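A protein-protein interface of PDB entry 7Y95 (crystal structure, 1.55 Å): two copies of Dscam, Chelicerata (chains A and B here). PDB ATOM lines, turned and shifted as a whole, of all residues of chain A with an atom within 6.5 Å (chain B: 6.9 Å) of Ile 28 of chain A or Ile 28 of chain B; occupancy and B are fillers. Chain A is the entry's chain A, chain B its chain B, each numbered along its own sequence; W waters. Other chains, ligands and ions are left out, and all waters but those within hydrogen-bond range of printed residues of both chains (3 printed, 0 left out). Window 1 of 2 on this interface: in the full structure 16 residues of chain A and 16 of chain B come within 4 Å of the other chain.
Water W2 lies within hydrogen-bond range of O of Phe 14 of chain A (2.7 Å) and NE2 of Gln 11 of chain B (3.2 Å).
Water W1 bridges NZ of Lys 26 of chain B (2.9 Å) and O of Asp 62 of chain A (2.9 Å).
Water W3 bridges the side-chain carboxylate (OD2) of Asp 62 of chain A (3.3 Å) and the side-chain amino group (NZ) of Lys 26 of chain B (3.4 Å).
Among the printed residues, merely in contact across the chains: Ile 28 of chain A with Ile 28 of chain B (3.4 Å), Leu 65 of chain A with Tyr 63 of chain B (3.6 Å), Tyr 63 of chain A with Leu 65 of chain B (3.7 Å), Lys 26 of chain A with Asn 30 of chain B (3.8 Å), Lys 26 of chain A with Ile 28 of chain B (3.8 Å), Asn 30 of chain A with Lys 26 of chain B (3.8 Å) and Tyr 63 of chain A with Lys 26 of chain B (3.9 Å).
Of the 17 printed residues of chain A, 7 touch a printed residue of chain B.
Of the 16 printed residues of chain B, 6 touch a printed residue of chain A.
Hydrophobic or aromatic side chains of chain B that line the printed part of chain A: Ile 28, Tyr 63 and Leu 65.
Among the printed residues, Asp or Glu carboxylates within 4 Å of a Lys or Arg side-chain nitrogen of the other chain: Asp 62 of chain A with Lys 26 of chain B (2.9 Å).
Gln 11 of chain A touches Lys 26 of chain B, and with the chains exchanged Lys 26 of chain A touches Gln 11 of chain B.
Lys 26 of chain A touches Ile 28 of chain B, but with the chains exchanged Ile 28 of chain A does not touch Lys 26 of chain B (5.0 Å).
Ile 28 of chain A touches its own counterpart, Ile 28 of chain B.
Tyr 63 of chain A touches its own counterpart, Tyr 63 of chain B.
Positions printed for both chains: 10, 11, 12, 13, 14, 26, 27, 28, 29, 30, 42, 63, 64, 65 and 66.
Of the 11 pairs that touch across the chains among the printed residues, 8 have their exchanged pair printed and touching as well.
O of Asn 30 of chain B is in hydrogen-bond range of N of Gln 11 of chain B, at 2.9 Å.
O of Asn 30 of chain A sits at hydrogen-bond distance from N of Gln 11 of chain A.
SG of Cys 81 of chain B forms a disulfide with SG of Cys 29 of chain B, 2.0 Å away.
O of Lys 58 of chain A lies within hydrogen-bond range of N of Leu 65 of chain A (2.8 Å).
The side-chain amide nitrogen (NE2) of Gln 11 of chain A is in hydrogen-bond range of the backbone carbonyl oxygen (O) of Lys 26 of chain B (2.7 Å).
The side-chain amino group (NZ) of Lys 26 of chain B is in salt-bridge range of the side-chain carboxylate (OD2) of Asp 62 of chain A (2.9 Å).
The side-chain amide nitrogen of Gln 11 of chain B sits at hydrogen-bond distance from the backbone carbonyl oxygen of Lys 26 of chain A.
The side-chain hydroxyl (OH) of Tyr 63 of chain B sits at hydrogen-bond distance from the side-chain hydroxyl (OH) of Tyr 63 of chain A.
Of chain B, only Ile 28 (3.4 Å) comes within 4 Å of Ile 28 of chain A.
Printed residues of chain B within 4 Å of Asp 62 of chain A: Lys 26 (2.9 Å).
Printed residues of chain B within 4 Å of Tyr 63 of chain A: Lys 26, Tyr 63 and Leu 65.
Of chain A, only Lys 26 (3.8 Å) and Ile 28 (3.4 Å) come within 4 Å of Ile 28 of chain B.
Of the printed residues of chain A, Leu 65 of chain B touches Tyr 63 (3.7 Å).
Cys 81 of chain B touches none of the printed residues of chain A.
The nearest residue of chain B that does not touch Ile 28 of chain A is Lys 26 of chain B (5.0 Å).
The nearest residue of chain A that does not touch Ile 28 of chain B is Leu 65 of chain A (4.02 Å).
The nearest printed residue of chain B that does not touch Gln 11 of chain A is Val 27 of chain B (4.9 Å).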
ATOM      1  N   ILE A  10      -0.511   0.687  12.255  1.00  0.00           N
ATOM      2  CA  ILE A  10      -1.799   0.763  12.928  1.00  0.00           C
ATOM      3  C   ILE A  10      -1.626   0.312  14.363  1.00  0.00           C
ATOM      4  O   ILE A  10      -0.933  -0.671  14.646  1.00  0.00           O
ATOM      5  CB  ILE A  10      -2.852  -0.097  12.211  1.00  0.00           C
ATOM      6  CG1 ILE A  10      -3.311   0.557  10.908  1.00  0.00           C
ATOM      7  CG2 ILE A  10      -4.081  -0.304  13.083  1.00  0.00           C
ATOM      8  CD1 ILE A  10      -4.257  -0.312  10.094  1.00  0.00           C
ATOM      9  N   GLN A  11      -2.264   1.025  15.268  1.00  0.00           N
ATOM     10  CA  GLN A  11      -2.411   0.569  16.647  1.00  0.00           C
ATOM     11  C   GLN A  11      -3.406  -0.587  16.672  1.00  0.00           C
ATOM     12  O   GLN A  11      -4.531  -0.431  16.175  1.00  0.00           O
ATOM     13  CB  GLN A  11      -2.897   1.723  17.526  1.00  0.00           C
ATOM     14  CG  GLN A  11      -3.198   1.312  18.939  1.00  0.00           C
ATOM     15  CD  GLN A  11      -3.683   2.473  19.792  1.00  0.00           C
ATOM     16  OE1 GLN A  11      -3.093   3.548  19.789  1.00  0.00           O
ATOM     17  NE2 GLN A  11      -4.741   2.244  20.552  1.00  0.00           N
ATOM     18  N   PRO A  12      -3.048  -1.748  17.205  1.00  0.00           N
ATOM     19  CA  PRO A  12      -3.993  -2.873  17.187  1.00  0.00           C
ATOM     20  C   PRO A  12      -5.252  -2.544  17.975  1.00  0.00           C
ATOM     21  O   PRO A  12      -5.189  -2.023  19.088  1.00  0.00           O
ATOM     22  CB  PRO A  12      -3.205  -4.022  17.830  1.00  0.00           C
ATOM     23  CG  PRO A  12      -1.789  -3.604  17.790  1.00  0.00           C
ATOM     24  CD  PRO A  12      -1.760  -2.105  17.830  1.00  0.00           C
ATOM     25  N   PHE A  13      -6.400  -2.858  17.388  1.00  0.00           N
ATOM     26  CA  PHE A  13      -7.685  -2.718  18.052  1.00  0.00           C
ATOM     27  C   PHE A  13      -8.401  -4.067  18.061  1.00  0.00           C
ATOM     28  O   PHE A  13      -8.205  -4.905  17.172  1.00  0.00           O
ATOM     29  CB  PHE A  13      -8.568  -1.638  17.369  1.00  0.00           C
ATOM     30  CG  PHE A  13      -8.858  -1.913  15.917  1.00  0.00           C
ATOM     31  CD1 PHE A  13      -9.901  -2.744  15.546  1.00  0.00           C
ATOM     32  CD2 PHE A  13      -8.094  -1.329  14.929  1.00  0.00           C
ATOM     33  CE1 PHE A  13     -10.165  -3.003  14.215  1.00  0.00           C
ATOM     34  CE2 PHE A  13      -8.346  -1.588  13.595  1.00  0.00           C
ATOM     35  CZ  PHE A  13      -9.382  -2.432  13.236  1.00  0.00           C
ATOM     36  N   PHE A  14      -9.192  -4.291  19.107  1.00  0.00           N
ATOM     37  CA  PHE A  14      -9.942  -5.525  19.266  1.00  0.00           C
ATOM     38  C   PHE A  14     -11.328  -5.217  19.813  1.00  0.00           C
ATOM     39  O   PHE A  14     -11.533  -4.217  20.509  1.00  0.00           O
ATOM     40  CB  PHE A  14      -9.205  -6.493  20.195  1.00  0.00           C
ATOM     41  CG  PHE A  14      -7.808  -6.796  19.736  1.00  0.00           C
ATOM     42  CD1 PHE A  14      -7.590  -7.629  18.657  1.00  0.00           C
ATOM     43  CD2 PHE A  14      -6.728  -6.184  20.326  1.00  0.00           C
ATOM     44  CE1 PHE A  14      -6.309  -7.888  18.212  1.00  0.00           C
ATOM     45  CE2 PHE A  14      -5.449  -6.428  19.872  1.00  0.00           C
ATOM     46  CZ  PHE A  14      -5.242  -7.283  18.815  1.00  0.00           C
ATOM     47  N   LYS A  26     -17.977   0.357  19.887  1.00  0.00           N
ATOM     48  CA  LYS A  26     -17.137   1.275  19.135  1.00  0.00           C
ATOM     49  C   LYS A  26     -15.714   0.749  19.101  1.00  0.00           C
ATOM     50  O   LYS A  26     -15.223   0.205  20.093  1.00  0.00           O
ATOM     51  CB  LYS A  26     -17.125   2.670  19.767  1.00  0.00           C
ATOM     52  CG  LYS A  26     -18.366   3.497  19.536  1.00  0.00           C
ATOM     53  CD  LYS A  26     -18.209   4.873  20.159  1.00  0.00           C
ATOM     54  CE  LYS A  26     -19.293   5.831  19.658  1.00  0.00           C
ATOM     55  NZ  LYS A  26     -20.665   5.319  19.947  1.00  0.00           N
ATOM     56  N   VAL A  27     -15.039   0.936  17.970  1.00  0.00           N
ATOM     57  CA  VAL A  27     -13.600   0.704  17.899  1.00  0.00           C
ATOM     58  C   VAL A  27     -12.984   1.861  17.127  1.00  0.00           C
ATOM     59  O   VAL A  27     -13.640   2.504  16.304  1.00  0.00           O
ATOM     60  CB  VAL A  27     -13.205  -0.651  17.257  1.00  0.00           C
ATOM     61  CG1 VAL A  27     -13.580  -1.806  18.179  1.00  0.00           C
ATOM     62  CG2 VAL A  27     -13.817  -0.810  15.886  1.00  0.00           C
ATOM     63  N   ILE A  28     -11.709   2.123  17.408  1.00  0.00           N
ATOM     64  CA  ILE A  28     -10.944   3.188  16.778  1.00  0.00           C
ATOM     65  C   ILE A  28      -9.787   2.564  16.013  1.00  0.00           C
ATOM     66  O   ILE A  28      -9.146   1.625  16.495  1.00  0.00           O
ATOM     67  CB  ILE A  28     -10.418   4.192  17.827  1.00  0.00           C
ATOM     68  CG1 ILE A  28     -11.528   5.148  18.272  1.00  0.00           C
ATOM     69  CG2 ILE A  28      -9.237   4.974  17.282  1.00  0.00           C
ATOM     70  CD1 ILE A  28     -12.257   5.822  17.157  1.00  0.00           C
ATOM     71  N   CYS A  29      -9.529   3.085  14.816  1.00  0.00           N
ATOM     72  CA  CYS A  29      -8.335   2.774  14.042  1.00  0.00           C
ATOM     73  C   CYS A  29      -7.473   4.027  14.005  1.00  0.00           C
ATOM     74  O   CYS A  29      -7.968   5.116  13.686  1.00  0.00           O
ATOM     75  CB  CYS A  29      -8.695   2.345  12.622  1.00  0.00           C
ATOM     76  SG  CYS A  29      -7.242   1.993  11.584  1.00  0.00           S
ATOM     77  N   ASN A  30      -6.207   3.894  14.384  1.00  0.00           N
ATOM     78  CA  ASN A  30      -5.344   5.064  14.391  1.00  0.00           C
ATOM     79  C   ASN A  30      -3.900   4.636  14.211  1.00  0.00           C
ATOM     80  O   ASN A  30      -3.527   3.523  14.605  1.00  0.00           O
ATOM     81  CB  ASN A  30      -5.495   5.880  15.688  1.00  0.00           C
ATOM     82  CG  ASN A  30      -5.067   5.112  16.919  1.00  0.00           C
ATOM     83  OD1 ASN A  30      -5.845   4.336  17.473  1.00  0.00           O
ATOM     84  ND2 ASN A  30      -3.827   5.334  17.362  1.00  0.00           N
ATOM     85  N   TRP A  42     -12.605   1.053   5.981  1.00  0.00           N
ATOM     86  CA  TRP A  42     -13.116  -0.032   6.803  1.00  0.00           C
ATOM     87  C   TRP A  42     -13.741  -1.102   5.924  1.00  0.00           C
ATOM     88  O   TRP A  42     -14.545  -0.796   5.039  1.00  0.00           O
ATOM     89  CB  TRP A  42     -14.159   0.468   7.802  1.00  0.00           C
ATOM     90  CG  TRP A  42     -13.608   1.275   8.933  1.00  0.00           C
ATOM     91  CD1 TRP A  42     -13.525   2.636   9.003  1.00  0.00           C
ATOM     92  CD2 TRP A  42     -13.084   0.776  10.164  1.00  0.00           C
ATOM     93  NE1 TRP A  42     -12.976   3.014  10.198  1.00  0.00           N
ATOM     94  CE2 TRP A  42     -12.695   1.890  10.931  1.00  0.00           C
ATOM     95  CE3 TRP A  42     -12.891  -0.506  10.687  1.00  0.00           C
ATOM     96  CZ2 TRP A  42     -12.125   1.763  12.197  1.00  0.00           C
ATOM     97  CZ3 TRP A  42     -12.337  -0.631  11.952  1.00  0.00           C
ATOM     98  CH2 TRP A  42     -11.964   0.502  12.693  1.00  0.00           C
ATOM     99  N   LYS A  58     -16.892   7.522  11.267  1.00  0.00           N
ATOM    100  CA  LYS A  58     -16.537   8.931  11.410  1.00  0.00           C
ATOM    101  C   LYS A  58     -15.021   9.038  11.388  1.00  0.00           C
ATOM    102  O   LYS A  58     -14.344   8.560  12.305  1.00  0.00           O
ATOM    103  CB  LYS A  58     -17.106   9.523  12.698  1.00  0.00           C
ATOM    104  CG  LYS A  58     -16.668  10.968  12.975  1.00  0.00           C
ATOM    105  CD  LYS A  58     -16.921  11.888  11.777  1.00  0.00           C
ATOM    106  CE  LYS A  58     -17.139  13.325  12.210  1.00  0.00           C
ATOM    107  NZ  LYS A  58     -18.081  14.053  11.305  1.00  0.00           N
ATOM    108  N   ASP A  62      -6.456  11.891  12.096  1.00  0.00           N
ATOM    109  CA  ASP A  62      -5.503  10.903  12.602  1.00  0.00           C
ATOM    110  C   ASP A  62      -6.173   9.724  13.307  1.00  0.00           C
ATOM    111  O   ASP A  62      -5.491   8.949  13.997  1.00  0.00           O
ATOM    112  CB  ASP A  62      -4.494  11.575  13.537  1.00  0.00           C
ATOM    113  CG  ASP A  62      -5.136  12.131  14.789  1.00  0.00           C
ATOM    114  OD1 ASP A  62      -6.378  12.202  14.848  1.00  0.00           O
ATOM    115  OD2 ASP A  62      -4.384  12.499  15.721  1.00  0.00           O
ATOM    116  N   TYR A  63      -7.474   9.535  13.112  1.00  0.00           N
ATOM    117  CA  TYR A  63      -8.134   8.318  13.559  1.00  0.00           C
ATOM    118  C   TYR A  63      -9.475   8.188  12.865  1.00  0.00           C
ATOM    119  O   TYR A  63      -9.982   9.146  12.283  1.00  0.00           O
ATOM    120  CB  TYR A  63      -8.305   8.283  15.085  1.00  0.00           C
ATOM    121  CG  TYR A  63      -9.364   9.202  15.688  1.00  0.00           C
ATOM    122  CD1 TYR A  63      -9.090  10.542  15.936  1.00  0.00           C
ATOM    123  CD2 TYR A  63     -10.608   8.708  16.059  1.00  0.00           C
ATOM    124  CE1 TYR A  63     -10.046  11.377  16.515  1.00  0.00           C
ATOM    125  CE2 TYR A  63     -11.569   9.530  16.637  1.00  0.00           C
ATOM    126  CZ  TYR A  63     -11.271  10.862  16.868  1.00  0.00           C
ATOM    127  OH  TYR A  63     -12.204  11.694  17.448  1.00  0.00           O
ATOM    128  N   SER A  64     -10.022   6.972  12.899  1.00  0.00           N
ATOM    129  CA  SER A  64     -11.336   6.688  12.341  1.00  0.00           C
ATOM    130  C   SER A  64     -12.113   5.832  13.327  1.00  0.00           C
ATOM    131  O   SER A  64     -11.566   4.905  13.928  1.00  0.00           O
ATOM    132  CB  SER A  64     -11.238   5.989  10.977  1.00  0.00           C
ATOM    133  OG  SER A  64     -12.518   5.786  10.401  1.00  0.00           O
ATOM    134  N   LEU A  65     -13.384   6.162  13.498  1.00  0.00           N
ATOM    135  CA  LEU A  65     -14.244   5.537  14.487  1.00  0.00           C
ATOM    136  C   LEU A  65     -15.331   4.740  13.782  1.00  0.00           C
ATOM    137  O   LEU A  65     -16.060   5.276  12.943  1.00  0.00           O
ATOM    138  CB  LEU A  65     -14.869   6.602  15.393  1.00  0.00           C
ATOM    139  CG  LEU A  65     -15.991   6.178  16.344  1.00  0.00           C
ATOM    140  CD1 LEU A  65     -15.485   5.276  17.437  1.00  0.00           C
ATOM    141  CD2 LEU A  65     -16.647   7.416  16.946  1.00  0.00           C
ATOM    142  N   LEU A  66     -15.436   3.467  14.138  1.00  0.00           N
ATOM    143  CA  LEU A  66     -16.509   2.587  13.700  1.00  0.00           C
ATOM    144  C   LEU A  66     -17.484   2.411  14.857  1.00  0.00           C
ATOM    145  O   LEU A  66     -17.088   1.997  15.953  1.00  0.00           O
ATOM    146  CB  LEU A  66     -15.945   1.236  13.262  1.00  0.00           C
ATOM    147  CG  LEU A  66     -16.979   0.161  12.936  1.00  0.00           C
ATOM    148  CD1 LEU A  66     -17.699   0.520  11.675  1.00  0.00           C
ATOM    149  CD2 LEU A  66     -16.292  -1.196  12.796  1.00  0.00           C
ATOM    150  N   ILE B  10     -19.461   1.200  30.779  1.00  0.00           N
ATOM    151  CA  ILE B  10     -18.364   1.492  29.863  1.00  0.00           C
ATOM    152  C   ILE B  10     -17.949   0.217  29.149  1.00  0.00           C
ATOM    153  O   ILE B  10     -17.834  -0.850  29.761  1.00  0.00           O
ATOM    154  CB  ILE B  10     -17.173   2.100  30.626  1.00  0.00           C
ATOM    155  CG1 ILE B  10     -17.535   3.449  31.231  1.00  0.00           C
ATOM    156  CG2 ILE B  10     -15.940   2.213  29.718  1.00  0.00           C
ATOM    157  CD1 ILE B  10     -16.494   3.958  32.203  1.00  0.00           C
ATOM    158  N   GLN B  11     -17.711   0.334  27.855  1.00  0.00           N
ATOM    159  CA  GLN B  11     -17.079  -0.737  27.091  1.00  0.00           C
ATOM    160  C   GLN B  11     -15.647  -0.896  27.582  1.00  0.00           C
ATOM    161  O   GLN B  11     -14.886   0.080  27.557  1.00  0.00           O
ATOM    162  CB  GLN B  11     -17.108  -0.406  25.598  1.00  0.00           C
ATOM    163  CG  GLN B  11     -16.368  -1.395  24.711  1.00  0.00           C
ATOM    164  CD  GLN B  11     -16.414  -0.977  23.253  1.00  0.00           C
ATOM    165  OE1 GLN B  11     -17.438  -0.504  22.768  1.00  0.00           O
ATOM    166  NE2 GLN B  11     -15.309  -1.161  22.547  1.00  0.00           N
ATOM    167  N   PRO B  12     -15.237  -2.072  28.045  1.00  0.00           N
ATOM    168  CA  PRO B  12     -13.867  -2.202  28.558  1.00  0.00           C
ATOM    169  C   PRO B  12     -12.855  -1.798  27.499  1.00  0.00           C
ATOM    170  O   PRO B  12     -12.932  -2.237  26.347  1.00  0.00           O
ATOM    171  CB  PRO B  12     -13.754  -3.688  28.918  1.00  0.00           C
ATOM    172  CG  PRO B  12     -15.160  -4.122  29.177  1.00  0.00           C
ATOM    173  CD  PRO B  12     -16.015  -3.315  28.207  1.00  0.00           C
ATOM    174  N   PHE B  13     -11.922  -0.930  27.890  1.00  0.00           N
ATOM    175  CA  PHE B  13     -10.836  -0.509  27.019  1.00  0.00           C
ATOM    176  C   PHE B  13      -9.494  -0.896  27.630  1.00  0.00           C
ATOM    177  O   PHE B  13      -9.367  -1.092  28.843  1.00  0.00           O
ATOM    178  CB  PHE B  13     -10.899   1.006  26.737  1.00  0.00           C
ATOM    179  CG  PHE B  13     -10.764   1.858  27.955  1.00  0.00           C
ATOM    180  CD1 PHE B  13      -9.523   2.152  28.483  1.00  0.00           C
ATOM    181  CD2 PHE B  13     -11.884   2.380  28.568  1.00  0.00           C
ATOM    182  CE1 PHE B  13      -9.402   2.938  29.603  1.00  0.00           C
ATOM    183  CE2 PHE B  13     -11.766   3.163  29.696  1.00  0.00           C
ATOM    184  CZ  PHE B  13     -10.527   3.451  30.205  1.00  0.00           C
ATOM    185  N   PHE B  14      -8.497  -1.052  26.763  1.00  0.00           N
ATOM    186  CA  PHE B  14      -7.167  -1.450  27.186  1.00  0.00           C
ATOM    187  C   PHE B  14      -6.154  -0.749  26.301  1.00  0.00           C
ATOM    188  O   PHE B  14      -6.470  -0.313  25.191  1.00  0.00           O
ATOM    189  CB  PHE B  14      -7.007  -2.969  27.109  1.00  0.00           C
ATOM    190  CG  PHE B  14      -8.051  -3.715  27.890  1.00  0.00           C
ATOM    191  CD1 PHE B  14      -7.898  -3.929  29.253  1.00  0.00           C
ATOM    192  CD2 PHE B  14      -9.202  -4.173  27.272  1.00  0.00           C
ATOM    193  CE1 PHE B  14      -8.875  -4.596  29.982  1.00  0.00           C
ATOM    194  CE2 PHE B  14     -10.175  -4.844  27.992  1.00  0.00           C
ATOM    195  CZ  PHE B  14     -10.015  -5.052  29.345  1.00  0.00           C
ATOM    196  N   LYS B  26      -3.821   6.124  21.387  1.00  0.00           N
ATOM    197  CA  LYS B  26      -5.176   6.615  21.588  1.00  0.00           C
ATOM    198  C   LYS B  26      -6.026   5.523  22.219  1.00  0.00           C
ATOM    199  O   LYS B  26      -5.940   4.354  21.833  1.00  0.00           O
ATOM    200  CB  LYS B  26      -5.821   7.042  20.259  1.00  0.00           C
ATOM    201  CG  LYS B  26      -5.252   8.302  19.653  1.00  0.00           C
ATOM    202  CD  LYS B  26      -5.950   8.624  18.333  1.00  0.00           C
ATOM    203  CE  LYS B  26      -5.729  10.064  17.921  1.00  0.00           C
ATOM    204  NZ  LYS B  26      -4.282  10.373  17.738  1.00  0.00           N
ATOM    205  N   VAL B  27      -6.863   5.906  23.175  1.00  0.00           N
ATOM    206  CA  VAL B  27      -7.895   5.025  23.705  1.00  0.00           C
ATOM    207  C   VAL B  27      -9.179   5.830  23.771  1.00  0.00           C
ATOM    208  O   VAL B  27      -9.160   7.045  23.999  1.00  0.00           O
ATOM    209  CB  VAL B  27      -7.549   4.434  25.089  1.00  0.00           C
ATOM    210  CG1 VAL B  27      -6.370   3.482  24.969  1.00  0.00           C
ATOM    211  CG2 VAL B  27      -7.260   5.530  26.085  1.00  0.00           C
ATOM    212  N   ILE B  28     -10.299   5.159  23.525  1.00  0.00           N
ATOM    213  CA  ILE B  28     -11.605   5.790  23.650  1.00  0.00           C
ATOM    214  C   ILE B  28     -12.380   5.125  24.775  1.00  0.00           C
ATOM    215  O   ILE B  28     -12.332   3.903  24.957  1.00  0.00           O
ATOM    216  CB  ILE B  28     -12.436   5.774  22.346  1.00  0.00           C
ATOM    217  CG1 ILE B  28     -12.613   4.367  21.793  1.00  0.00           C
ATOM    218  CG2 ILE B  28     -11.811   6.716  21.295  1.00  0.00           C
ATOM    219  CD1 ILE B  28     -13.899   4.226  20.981  1.00  0.00           C
ATOM    220  N   CYS B  29     -13.100   5.949  25.524  1.00  0.00           N
ATOM    221  CA  CYS B  29     -14.079   5.513  26.499  1.00  0.00           C
ATOM    222  C   CYS B  29     -15.458   5.750  25.912  1.00  0.00           C
ATOM    223  O   CYS B  29     -15.744   6.850  25.426  1.00  0.00           O
ATOM    224  CB  CYS B  29     -13.888   6.297  27.780  1.00  0.00           C
ATOM    225  SG  CYS B  29     -15.067   5.957  29.045  1.00  0.00           S
ATOM    226  N   ASN B  30     -16.293   4.716  25.900  1.00  0.00           N
ATOM    227  CA  ASN B  30     -17.643   4.883  25.392  1.00  0.00           C
ATOM    228  C   ASN B  30     -18.584   3.937  26.113  1.00  0.00           C
ATOM    229  O   ASN B  30     -18.147   2.906  26.640  1.00  0.00           O
ATOM    230  CB  ASN B  30     -17.703   4.635  23.880  1.00  0.00           C
ATOM    231  CG  ASN B  30     -17.309   3.218  23.513  1.00  0.00           C
ATOM    232  OD1 ASN B  30     -16.127   2.915  23.380  1.00  0.00           O
ATOM    233  ND2 ASN B  30     -18.309   2.343  23.331  1.00  0.00           N
ATOM    234  N   TRP B  42     -11.448  11.692  32.781  1.00  0.00           N
ATOM    235  CA  TRP B  42     -10.292  10.812  32.766  1.00  0.00           C
ATOM    236  C   TRP B  42      -9.434  11.048  34.000  1.00  0.00           C
ATOM    237  O   TRP B  42      -9.164  12.196  34.372  1.00  0.00           O
ATOM    238  CB  TRP B  42      -9.442  11.029  31.512  1.00  0.00           C
ATOM    239  CG  TRP B  42     -10.042  10.494  30.259  1.00  0.00           C
ATOM    240  CD1 TRP B  42     -10.812  11.178  29.361  1.00  0.00           C
ATOM    241  CD2 TRP B  42      -9.918   9.162  29.744  1.00  0.00           C
ATOM    242  NE1 TRP B  42     -11.167  10.359  28.324  1.00  0.00           N
ATOM    243  CE2 TRP B  42     -10.639   9.113  28.536  1.00  0.00           C
ATOM    244  CE3 TRP B  42      -9.275   8.005  30.191  1.00  0.00           C
ATOM    245  CZ2 TRP B  42     -10.735   7.954  27.767  1.00  0.00           C
ATOM    246  CZ3 TRP B  42      -9.373   6.855  29.431  1.00  0.00           C
ATOM    247  CH2 TRP B  42     -10.083   6.841  28.224  1.00  0.00           C
ATOM    248  N   TYR B  63     -18.612   9.513  23.347  1.00  0.00           N
ATOM    249  CA  TYR B  63     -17.324   8.900  23.627  1.00  0.00           C
ATOM    250  C   TYR B  63     -16.346   9.992  24.018  1.00  0.00           C
ATOM    251  O   TYR B  63     -16.565  11.175  23.743  1.00  0.00           O
ATOM    252  CB  TYR B  63     -16.791   8.100  22.428  1.00  0.00           C
ATOM    253  CG  TYR B  63     -16.260   8.911  21.255  1.00  0.00           C
ATOM    254  CD1 TYR B  63     -17.117   9.429  20.296  1.00  0.00           C
ATOM    255  CD2 TYR B  63     -14.901   9.128  21.097  1.00  0.00           C
ATOM    256  CE1 TYR B  63     -16.632  10.150  19.223  1.00  0.00           C
ATOM    257  CE2 TYR B  63     -14.406   9.840  20.030  1.00  0.00           C
ATOM    258  CZ  TYR B  63     -15.271  10.356  19.098  1.00  0.00           C
ATOM    259  OH  TYR B  63     -14.763  11.064  18.022  1.00  0.00           O
ATOM    260  N   SER B  64     -15.251   9.575  24.644  1.00  0.00           N
ATOM    261  CA  SER B  64     -14.170  10.482  24.987  1.00  0.00           C
ATOM    262  C   SER B  64     -12.854   9.854  24.560  1.00  0.00           C
ATOM    263  O   SER B  64     -12.625   8.659  24.763  1.00  0.00           O
ATOM    264  CB  SER B  64     -14.156  10.811  26.488  1.00  0.00           C
ATOM    265  OG  SER B  64     -13.147  11.752  26.775  1.00  0.00           O
ATOM    266  N   LEU B  65     -11.997  10.670  23.964  1.00  0.00           N
ATOM    267  CA  LEU B  65     -10.726  10.219  23.421  1.00  0.00           C
ATOM    268  C   LEU B  65      -9.585  10.712  24.299  1.00  0.00           C
ATOM    269  O   LEU B  65      -9.463  11.915  24.550  1.00  0.00           O
ATOM    270  CB  LEU B  65     -10.558  10.732  21.992  1.00  0.00           C
ATOM    271  CG  LEU B  65      -9.187  10.536  21.348  1.00  0.00           C
ATOM    272  CD1 LEU B  65      -8.936   9.071  21.066  1.00  0.00           C
ATOM    273  CD2 LEU B  65      -9.114  11.367  20.073  1.00  0.00           C
ATOM    274  N   LEU B  66      -8.751   9.785  24.757  1.00  0.00           N
ATOM    275  CA  LEU B  66      -7.477  10.111  25.380  1.00  0.00           C
ATOM    276  C   LEU B  66      -6.394   9.891  24.334  1.00  0.00           C
ATOM    277  O   LEU B  66      -6.274   8.789  23.790  1.00  0.00           O
ATOM    278  CB  LEU B  66      -7.235   9.244  26.611  1.00  0.00           C
ATOM    279  CG  LEU B  66      -5.893   9.438  27.303  1.00  0.00           C
ATOM    280  CD1 LEU B  66      -5.810  10.811  27.944  1.00  0.00           C
ATOM    281  CD2 LEU B  66      -5.671   8.339  28.345  1.00  0.00           C
ATOM    282  N   CYS B  81     -11.521   5.949  33.114  1.00  0.00           N
ATOM    283  CA  CYS B  81     -12.589   6.762  32.556  1.00  0.00           C
ATOM    284  C   CYS B  81     -13.789   6.643  33.482  1.00  0.00           C
ATOM    285  O   CYS B  81     -14.181   5.529  33.847  1.00  0.00           O
ATOM    286  CB  CYS B  81     -12.961   6.315  31.148  1.00  0.00           C
ATOM    287  SG  CYS B  81     -14.407   7.203  30.530  1.00  0.00           S
HETATM  288  O   HOH W   1      -3.144   8.728  15.691  1.00  0.00           O
HETATM  289  O   HOH W   2     -12.879  -3.301  22.619  1.00  0.00           O
HETATM  290  O   HOH W   3      -1.479  12.257  17.224  1.00  0.00           O
